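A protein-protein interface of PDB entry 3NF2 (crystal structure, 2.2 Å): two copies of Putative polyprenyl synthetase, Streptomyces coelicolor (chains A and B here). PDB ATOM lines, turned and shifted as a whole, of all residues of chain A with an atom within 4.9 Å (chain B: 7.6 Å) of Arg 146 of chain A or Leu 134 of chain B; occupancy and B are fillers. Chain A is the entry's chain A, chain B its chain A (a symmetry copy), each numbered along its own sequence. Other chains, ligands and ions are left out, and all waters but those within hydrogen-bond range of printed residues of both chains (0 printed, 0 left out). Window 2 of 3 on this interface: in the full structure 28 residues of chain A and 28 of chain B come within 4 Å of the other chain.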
ATOM      1  N   GLY A 142       1.598  20.817  17.234  1.00  0.00           N
ATOM      2  CA  GLY A 142       0.589  19.778  17.084  1.00  0.00           C
ATOM      3  C   GLY A 142       1.236  18.503  16.581  1.00  0.00           C
ATOM      4  O   GLY A 142       0.911  17.389  17.030  1.00  0.00           O
ATOM      5  N   ARG A 143       2.173  18.678  15.656  1.00  0.00           N
ATOM      6  CA  ARG A 143       2.913  17.561  15.086  1.00  0.00           C
ATOM      7  C   ARG A 143       3.874  16.953  16.109  1.00  0.00           C
ATOM      8  O   ARG A 143       4.067  15.739  16.145  1.00  0.00           O
ATOM      9  CB  ARG A 143       3.650  18.012  13.822  1.00  0.00           C
ATOM     10  CG  ARG A 143       2.807  17.921  12.547  1.00  0.00           C
ATOM     11  CD  ARG A 143       3.308  18.875  11.466  1.00  0.00           C
ATOM     12  NE  ARG A 143       4.746  19.108  11.564  1.00  0.00           N
ATOM     13  CZ  ARG A 143       5.386  20.159  11.049  1.00  0.00           C
ATOM     14  NH1 ARG A 143       4.719  21.104  10.377  1.00  0.00           N
ATOM     15  NH2 ARG A 143       6.705  20.270  11.213  1.00  0.00           N
ATOM     16  N   ALA A 144       4.454  17.802  16.947  1.00  0.00           N
ATOM     17  CA  ALA A 144       5.330  17.361  18.024  1.00  0.00           C
ATOM     18  C   ALA A 144       4.568  16.563  19.090  1.00  0.00           C
ATOM     19  O   ALA A 144       5.108  15.596  19.630  1.00  0.00           O
ATOM     20  CB  ALA A 144       6.039  18.549  18.649  1.00  0.00           C
ATOM     21  N   THR A 145       3.324  16.964  19.372  1.00  0.00           N
ATOM     22  CA  THR A 145       2.452  16.234  20.305  1.00  0.00           C
ATOM     23  C   THR A 145       2.062  14.865  19.733  1.00  0.00           C
ATOM     24  O   THR A 145       1.937  13.895  20.479  1.00  0.00           O
ATOM     25  CB  THR A 145       1.177  17.045  20.691  1.00  0.00           C
ATOM     26  OG1 THR A 145       1.527  18.402  20.975  1.00  0.00           O
ATOM     27  CG2 THR A 145       0.485  16.452  21.933  1.00  0.00           C
ATOM     28  N   ARG A 146       1.892  14.803  18.411  1.00  0.00           N
ATOM     29  CA  ARG A 146       1.618  13.560  17.675  1.00  0.00           C
ATOM     30  C   ARG A 146       2.732  12.534  17.896  1.00  0.00           C
ATOM     31  O   ARG A 146       2.465  11.347  18.095  1.00  0.00           O
ATOM     32  CB  ARG A 146       1.476  13.878  16.180  1.00  0.00           C
ATOM     33  CG  ARG A 146       1.373  12.691  15.232  1.00  0.00           C
ATOM     34  CD  ARG A 146      -0.023  12.558  14.679  1.00  0.00           C
ATOM     35  NE  ARG A 146      -0.224  11.294  13.972  1.00  0.00           N
ATOM     36  CZ  ARG A 146      -0.248  11.158  12.647  1.00  0.00           C
ATOM     37  NH1 ARG A 146      -0.075  12.214  11.859  1.00  0.00           N
ATOM     38  NH2 ARG A 146      -0.448   9.959  12.110  1.00  0.00           N
ATOM     39  N   ARG A 147       3.974  13.015  17.875  1.00  0.00           N
ATOM     40  CA  ARG A 147       5.157  12.192  18.088  1.00  0.00           C
ATOM     41  C   ARG A 147       5.251  11.738  19.533  1.00  0.00           C
ATOM     42  O   ARG A 147       5.698  10.629  19.807  1.00  0.00           O
ATOM     43  CB  ARG A 147       6.431  12.978  17.750  1.00  0.00           C
ATOM     44  CG  ARG A 147       6.489  13.558  16.349  1.00  0.00           C
ATOM     45  CD  ARG A 147       6.960  12.549  15.345  1.00  0.00           C
ATOM     46  NE  ARG A 147       6.756  13.019  13.980  1.00  0.00           N
ATOM     47  CZ  ARG A 147       7.281  12.440  12.907  1.00  0.00           C
ATOM     48  NH1 ARG A 147       8.056  11.370  13.043  1.00  0.00           N
ATOM     49  NH2 ARG A 147       7.036  12.935  11.700  1.00  0.00           N
ATOM     50  N   LEU A 148       4.852  12.618  20.451  1.00  0.00           N
ATOM     51  CA  LEU A 148       4.877  12.320  21.881  1.00  0.00           C
ATOM     52  C   LEU A 148       3.864  11.232  22.193  1.00  0.00           C
ATOM     53  O   LEU A 148       4.146  10.326  22.973  1.00  0.00           O
ATOM     54  CB  LEU A 148       4.563  13.575  22.697  1.00  0.00           C
ATOM     55  CG  LEU A 148       4.855  13.515  24.206  1.00  0.00           C
ATOM     56  CD1 LEU A 148       6.339  13.715  24.497  1.00  0.00           C
ATOM     57  CD2 LEU A 148       4.023  14.529  24.947  1.00  0.00           C
ATOM     58  N   THR A 149       2.700  11.331  21.553  1.00  0.00           N
ATOM     59  CA  THR A 149       1.607  10.382  21.732  1.00  0.00           C
ATOM     60  C   THR A 149       1.985   8.972  21.268  1.00  0.00           C
ATOM     61  O   THR A 149       1.680   8.003  21.946  1.00  0.00           O
ATOM     62  CB  THR A 149       0.328  10.869  21.011  1.00  0.00           C
ATOM     63  OG1 THR A 149       0.026  12.196  21.457  1.00  0.00           O
ATOM     64  CG2 THR A 149      -0.884   9.934  21.298  1.00  0.00           C
ATOM     65  N   LYS A 150       2.659   8.877  20.126  1.00  0.00           N
ATOM     66  CA  LYS A 150       3.122   7.606  19.592  1.00  0.00           C
ATOM     67  C   LYS A 150       4.069   6.937  20.589  1.00  0.00           C
ATOM     68  O   LYS A 150       3.924   5.746  20.887  1.00  0.00           O
ATOM     69  CB  LYS A 150       3.807   7.814  18.234  1.00  0.00           C
ATOM     70  CG  LYS A 150       4.423   6.541  17.634  1.00  0.00           C
ATOM     71  CD  LYS A 150       5.065   6.783  16.275  1.00  0.00           C
ATOM     72  CE  LYS A 150       5.696   5.502  15.738  1.00  0.00           C
ATOM     73  NZ  LYS A 150       5.793   5.514  14.255  1.00  0.00           N
ATOM     74  N   PRO B  78     -14.571  12.159  16.034  1.00  0.00           N
ATOM     75  CA  PRO B  78     -13.285  12.056  16.737  1.00  0.00           C
ATOM     76  C   PRO B  78     -13.300  12.747  18.099  1.00  0.00           C
ATOM     77  O   PRO B  78     -12.746  12.218  19.073  1.00  0.00           O
ATOM     78  CB  PRO B  78     -12.319  12.781  15.803  1.00  0.00           C
ATOM     79  CG  PRO B  78     -12.889  12.581  14.453  1.00  0.00           C
ATOM     80  CD  PRO B  78     -14.378  12.541  14.618  1.00  0.00           C
ATOM     81  N   ALA B 127      -3.939   8.007  26.397  1.00  0.00           N
ATOM     82  CA  ALA B 127      -3.054   8.169  25.240  1.00  0.00           C
ATOM     83  C   ALA B 127      -3.797   7.972  23.903  1.00  0.00           C
ATOM     84  O   ALA B 127      -3.518   8.674  22.921  1.00  0.00           O
ATOM     85  CB  ALA B 127      -1.859   7.247  25.337  1.00  0.00           C
ATOM     86  N   LEU B 128      -4.750   7.039  23.880  1.00  0.00           N
ATOM     87  CA  LEU B 128      -5.557   6.789  22.679  1.00  0.00           C
ATOM     88  C   LEU B 128      -6.442   7.979  22.282  1.00  0.00           C
ATOM     89  O   LEU B 128      -6.719   8.188  21.099  1.00  0.00           O
ATOM     90  CB  LEU B 128      -6.413   5.522  22.860  1.00  0.00           C
ATOM     91  CG  LEU B 128      -7.188   4.977  21.659  1.00  0.00           C
ATOM     92  CD1 LEU B 128      -6.290   4.649  20.434  1.00  0.00           C
ATOM     93  CD2 LEU B 128      -7.978   3.767  22.072  1.00  0.00           C
ATOM     94  N   ALA B 129      -6.880   8.742  23.280  1.00  0.00           N
ATOM     95  CA  ALA B 129      -7.772   9.878  23.069  1.00  0.00           C
ATOM     96  C   ALA B 129      -7.054  10.956  22.305  1.00  0.00           C
ATOM     97  O   ALA B 129      -7.604  11.527  21.360  1.00  0.00           O
ATOM     98  CB  ALA B 129      -8.280  10.424  24.404  1.00  0.00           C
ATOM     99  N   ASN B 130      -5.820  11.221  22.720  1.00  0.00           N
ATOM    100  CA  ASN B 130      -4.950  12.169  22.037  1.00  0.00           C
ATOM    101  C   ASN B 130      -4.616  11.711  20.623  1.00  0.00           C
ATOM    102  O   ASN B 130      -4.525  12.530  19.710  1.00  0.00           O
ATOM    103  CB  ASN B 130      -3.657  12.379  22.834  1.00  0.00           C
ATOM    104  CG  ASN B 130      -3.891  13.095  24.139  1.00  0.00           C
ATOM    105  OD1 ASN B 130      -4.668  14.036  24.210  1.00  0.00           O
ATOM    106  ND2 ASN B 130      -3.210  12.656  25.181  1.00  0.00           N
ATOM    107  N   GLU B 131      -4.450  10.400  20.457  1.00  0.00           N
ATOM    108  CA  GLU B 131      -4.175   9.795  19.160  1.00  0.00           C
ATOM    109  C   GLU B 131      -5.354   9.978  18.215  1.00  0.00           C
ATOM    110  O   GLU B 131      -5.172  10.369  17.072  1.00  0.00           O
ATOM    111  CB  GLU B 131      -3.880   8.302  19.315  1.00  0.00           C
ATOM    112  CG  GLU B 131      -3.363   7.619  18.062  1.00  0.00           C
ATOM    113  CD  GLU B 131      -1.855   7.754  17.909  1.00  0.00           C
ATOM    114  OE1 GLU B 131      -1.390   8.816  17.433  1.00  0.00           O
ATOM    115  OE2 GLU B 131      -1.133   6.792  18.261  1.00  0.00           O
ATOM    116  N   VAL B 132      -6.558   9.703  18.710  1.00  0.00           N
ATOM    117  CA  VAL B 132      -7.776   9.763  17.906  1.00  0.00           C
ATOM    118  C   VAL B 132      -7.986  11.147  17.275  1.00  0.00           C
ATOM    119  O   VAL B 132      -8.524  11.261  16.172  1.00  0.00           O
ATOM    120  CB  VAL B 132      -9.000   9.268  18.730  1.00  0.00           C
ATOM    121  CG1 VAL B 132     -10.318   9.915  18.294  1.00  0.00           C
ATOM    122  CG2 VAL B 132      -9.099   7.755  18.645  1.00  0.00           C
ATOM    123  N   LEU B 133      -7.513  12.185  17.958  1.00  0.00           N
ATOM    124  CA  LEU B 133      -7.573  13.542  17.429  1.00  0.00           C
ATOM    125  C   LEU B 133      -6.382  13.877  16.538  1.00  0.00           C
ATOM    126  O   LEU B 133      -6.566  14.327  15.415  1.00  0.00           O
ATOM    127  CB  LEU B 133      -7.699  14.568  18.564  1.00  0.00           C
ATOM    128  CG  LEU B 133      -8.998  14.493  19.375  1.00  0.00           C
ATOM    129  CD1 LEU B 133      -8.907  15.375  20.613  1.00  0.00           C
ATOM    130  CD2 LEU B 133     -10.211  14.870  18.514  1.00  0.00           C
ATOM    131  N   LEU B 134      -5.170  13.653  17.044  1.00  0.00           N
ATOM    132  CA  LEU B 134      -3.945  14.026  16.336  1.00  0.00           C
ATOM    133  C   LEU B 134      -3.700  13.227  15.039  1.00  0.00           C
ATOM    134  O   LEU B 134      -3.030  13.738  14.137  1.00  0.00           O
ATOM    135  CB  LEU B 134      -2.728  13.965  17.270  1.00  0.00           C
ATOM    136  CG  LEU B 134      -2.634  14.988  18.417  1.00  0.00           C
ATOM    137  CD1 LEU B 134      -1.769  14.473  19.559  1.00  0.00           C
ATOM    138  CD2 LEU B 134      -2.114  16.343  17.948  1.00  0.00           C
ATOM    139  N   GLU B 135      -4.272  12.014  14.947  1.00  0.00           N
ATOM    140  CA  GLU B 135      -4.286  11.177  13.724  1.00  0.00           C
ATOM    141  C   GLU B 135      -4.702  11.947  12.476  1.00  0.00           C
ATOM    142  O   GLU B 135      -4.242  11.639  11.373  1.00  0.00           O
ATOM    143  CB  GLU B 135      -5.248   9.979  13.862  1.00  0.00           C
ATOM    144  CG  GLU B 135      -4.597   8.690  14.291  1.00  0.00           C
ATOM    145  CD  GLU B 135      -5.575   7.530  14.521  1.00  0.00           C
ATOM    146  OE1 GLU B 135      -6.805   7.736  14.659  1.00  0.00           O
ATOM    147  OE2 GLU B 135      -5.087   6.382  14.579  1.00  0.00           O
ATOM    148  N   LEU B 136      -5.581  12.932  12.667  1.00  0.00           N
ATOM    149  CA  LEU B 136      -6.130  13.736  11.574  1.00  0.00           C
ATOM    150  C   LEU B 136      -5.087  14.621  10.884  1.00  0.00           C
ATOM    151  O   LEU B 136      -5.218  14.921   9.695  1.00  0.00           O
ATOM    152  CB  LEU B 136      -7.323  14.560  12.066  1.00  0.00           C
ATOM    153  CG  LEU B 136      -8.491  13.713  12.588  1.00  0.00           C
ATOM    154  CD1 LEU B 136      -9.478  14.555  13.378  1.00  0.00           C
ATOM    155  CD2 LEU B 136      -9.198  12.976  11.457  1.00  0.00           C
ATOM    156  N   GLY B 137      -4.055  15.021  11.628  1.00  0.00           N
ATOM    157  CA  GLY B 137      -2.923  15.759  11.067  1.00  0.00           C
ATOM    158  C   GLY B 137      -3.172  17.222  10.742  1.00  0.00           C
ATOM    159  O   GLY B 137      -2.270  17.909  10.259  1.00  0.00           O
ATOM    160  N   THR B 138      -4.384  17.701  11.025  1.00  0.00           N
ATOM    161  CA  THR B 138      -4.806  19.066  10.695  1.00  0.00           C
ATOM    162  C   THR B 138      -4.566  20.051  11.840  1.00  0.00           C
ATOM    163  O   THR B 138      -4.294  19.651  12.977  1.00  0.00           O
ATOM    164  CB  THR B 138      -6.307  19.115  10.288  1.00  0.00           C
ATOM    165  OG1 THR B 138      -7.122  18.651  11.373  1.00  0.00           O
ATOM    166  CG2 THR B 138      -6.566  18.245   9.058  1.00  0.00           C
ATOM    167  N   ALA B 141      -7.321  19.772  14.501  1.00  0.00           N
ATOM    168  CA  ALA B 141      -7.079  18.630  15.368  1.00  0.00           C
ATOM    169  C   ALA B 141      -6.100  18.940  16.501  1.00  0.00           C
ATOM    170  O   ALA B 141      -6.207  18.370  17.587  1.00  0.00           O
ATOM    171  CB  ALA B 141      -6.577  17.461  14.541  1.00  0.00           C
ATOM    172  N   GLY B 142      -5.148  19.831  16.238  1.00  0.00           N
ATOM    173  CA  GLY B 142      -4.172  20.245  17.237  1.00  0.00           C
ATOM    174  C   GLY B 142      -4.841  21.128  18.272  1.00  0.00           C
ATOM    175  O   GLY B 142      -4.582  21.019  19.484  1.00  0.00           O
ATOM    176  N   ARG B 143      -5.721  21.995  17.784  1.00  0.00           N
ATOM    177  CA  ARG B 143      -6.473  22.899  18.643  1.00  0.00           C
ATOM    178  C   ARG B 143      -7.508  22.141  19.474  1.00  0.00           C
ATOM    179  O   ARG B 143      -7.749  22.474  20.633  1.00  0.00           O
ATOM    180  CB  ARG B 143      -7.126  23.999  17.800  1.00  0.00           C
ATOM    181  CG  ARG B 143      -6.222  25.210  17.555  1.00  0.00           C
ATOM    182  CD  ARG B 143      -6.629  25.977  16.299  1.00  0.00           C
ATOM    183  NE  ARG B 143      -8.061  25.869  16.032  1.00  0.00           N
ATOM    184  CZ  ARG B 143      -8.632  26.073  14.843  1.00  0.00           C
ATOM    185  NH1 ARG B 143      -7.895  26.407  13.778  1.00  0.00           N
ATOM    186  NH2 ARG B 143      -9.953  25.933  14.719  1.00  0.00           N
ATOM    187  N   ALA B 144      -8.097  21.110  18.883  1.00  0.00           N
ATOM    188  CA  ALA B 144      -9.045  20.248  19.575  1.00  0.00           C
ATOM    189  C   ALA B 144      -8.371  19.439  20.690  1.00  0.00           C
ATOM    190  O   ALA B 144      -8.974  19.231  21.745  1.00  0.00           O
ATOM    191  CB  ALA B 144      -9.739  19.326  18.590  1.00  0.00           C
ATOM    192  N   THR B 145      -7.127  19.003  20.456  1.00  0.00           N
ATOM    193  CA  THR B 145      -6.333  18.296  21.473  1.00  0.00           C
ATOM    194  C   THR B 145      -5.967  19.234  22.630  1.00  0.00           C
ATOM    195  O   THR B 145      -5.918  18.807  23.783  1.00  0.00           O
ATOM    196  CB  THR B 145      -5.050  17.639  20.879  1.00  0.00           C
ATOM    197  OG1 THR B 145      -5.362  16.978  19.650  1.00  0.00           O
ATOM    198  CG2 THR B 145      -4.447  16.604  21.848  1.00  0.00           C
ATOM    199  N   ARG B 146      -5.731  20.507  22.308  1.00  0.00           N
ATOM    200  CA  ARG B 146      -5.467  21.568  23.290  1.00  0.00           C
ATOM    201  C   ARG B 146      -6.630  21.706  24.278  1.00  0.00           C
ATOM    202  O   ARG B 146      -6.419  21.859  25.482  1.00  0.00           O
ATOM    203  CB  ARG B 146      -5.236  22.895  22.553  1.00  0.00           C
ATOM    204  CG  ARG B 146      -5.130  24.148  23.412  1.00  0.00           C
ATOM    205  CD  ARG B 146      -3.713  24.662  23.448  1.00  0.00           C
ATOM    206  NE  ARG B 146      -3.524  25.705  24.455  1.00  0.00           N
ATOM    207  CZ  ARG B 146      -3.436  27.009  24.195  1.00  0.00           C
ATOM    208  NH1 ARG B 146      -3.528  27.453  22.946  1.00  0.00           N
ATOM    209  NH2 ARG B 146      -3.254  27.869  25.191  1.00  0.00           N
ATOM    210  N   LEU B 198     -13.138  21.240  15.539  1.00  0.00           N
ATOM    211  CA  LEU B 198     -12.846  20.306  14.445  1.00  0.00           C
ATOM    212  C   LEU B 198     -13.436  20.771  13.108  1.00  0.00           C
ATOM    213  O   LEU B 198     -12.924  20.423  12.041  1.00  0.00           O
ATOM    214  CB  LEU B 198     -13.334  18.889  14.791  1.00  0.00           C
ATOM    215  CG  LEU B 198     -12.526  18.091  15.829  1.00  0.00           C
ATOM    216  CD1 LEU B 198     -13.214  16.776  16.213  1.00  0.00           C
ATOM    217  CD2 LEU B 198     -11.096  17.827  15.351  1.00  0.00           C
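The backbone carbonyl oxygen (O) of Thr 145 of chain A is in hydrogen-bond range of the side-chain hydroxyl (OG1) of Thr 149 of chain A (2.7 Å).
Leu 134 of chain B touches Gly 142 of chain A (CD2 to O, 3.3 Å).
CD1 of Leu 134 of chain B touches CG2 of Thr 145 of chain A, at 3.8 Å.
CD of Arg 146 of chain A touches O of Leu 134 of chain B, at 3.3 Å.
Thr 149 of chain A touches Ala 127 of chain B.
Thr 149 of chain A touches Asn 130 of chain B (OG1 to CB, 3.9 Å).
Glu 131 of chain B touches Thr 149 of chain A.
CD1 of Leu 134 of chain B touches OG1 of Thr 149 of chain A, 3.5 Å away.
Of the printed residues of chain B, Gly 142 of chain A touches Leu 134 (3.3 Å).
Of the printed residues of chain B, Thr 145 of chain A touches Leu 134.
Of chain B, only Leu 134 (3.3 Å) comes within 4 Å of Arg 146 of chain A.
Printed residues of chain B within 4 Å of Thr 149 of chain A: Ala 127 (3.3 Å), Asn 130 (3.9 Å), Glu 131 (3.7 Å) and Leu 134 (3.5 Å).
Leu 128 of chain B touches none of the printed residues of chain A.
Of the printed residues of chain A, Asn 130 of chain B touches Thr 149.
Of the printed residues of chain A, Glu 131 of chain B touches Thr 149.
Leu 134 of chain B touches four residues of chain A.
The nearest printed residue of chain A that does not touch Glu 131 of chain B is Arg 146 of chain A (4.4 Å).
Of the 20 printed residues of chain B, 4 touch a printed residue of chain A.
Printed residues of chain B that touch a printed residue of chain A: Ala 127, Asn 130, Glu 131 and Leu 134.
Hydrophobic or aromatic side chains of chain B that line the printed part of chain A: Leu 134.
Along chain B the printed residues that touch a printed residue of chain A span positions 127 to 134.
Printed residues of chain A that touch a printed residue of chain B: Gly 142, Thr 145, Arg 146 and Thr 149.
5 positions are printed for both chains.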
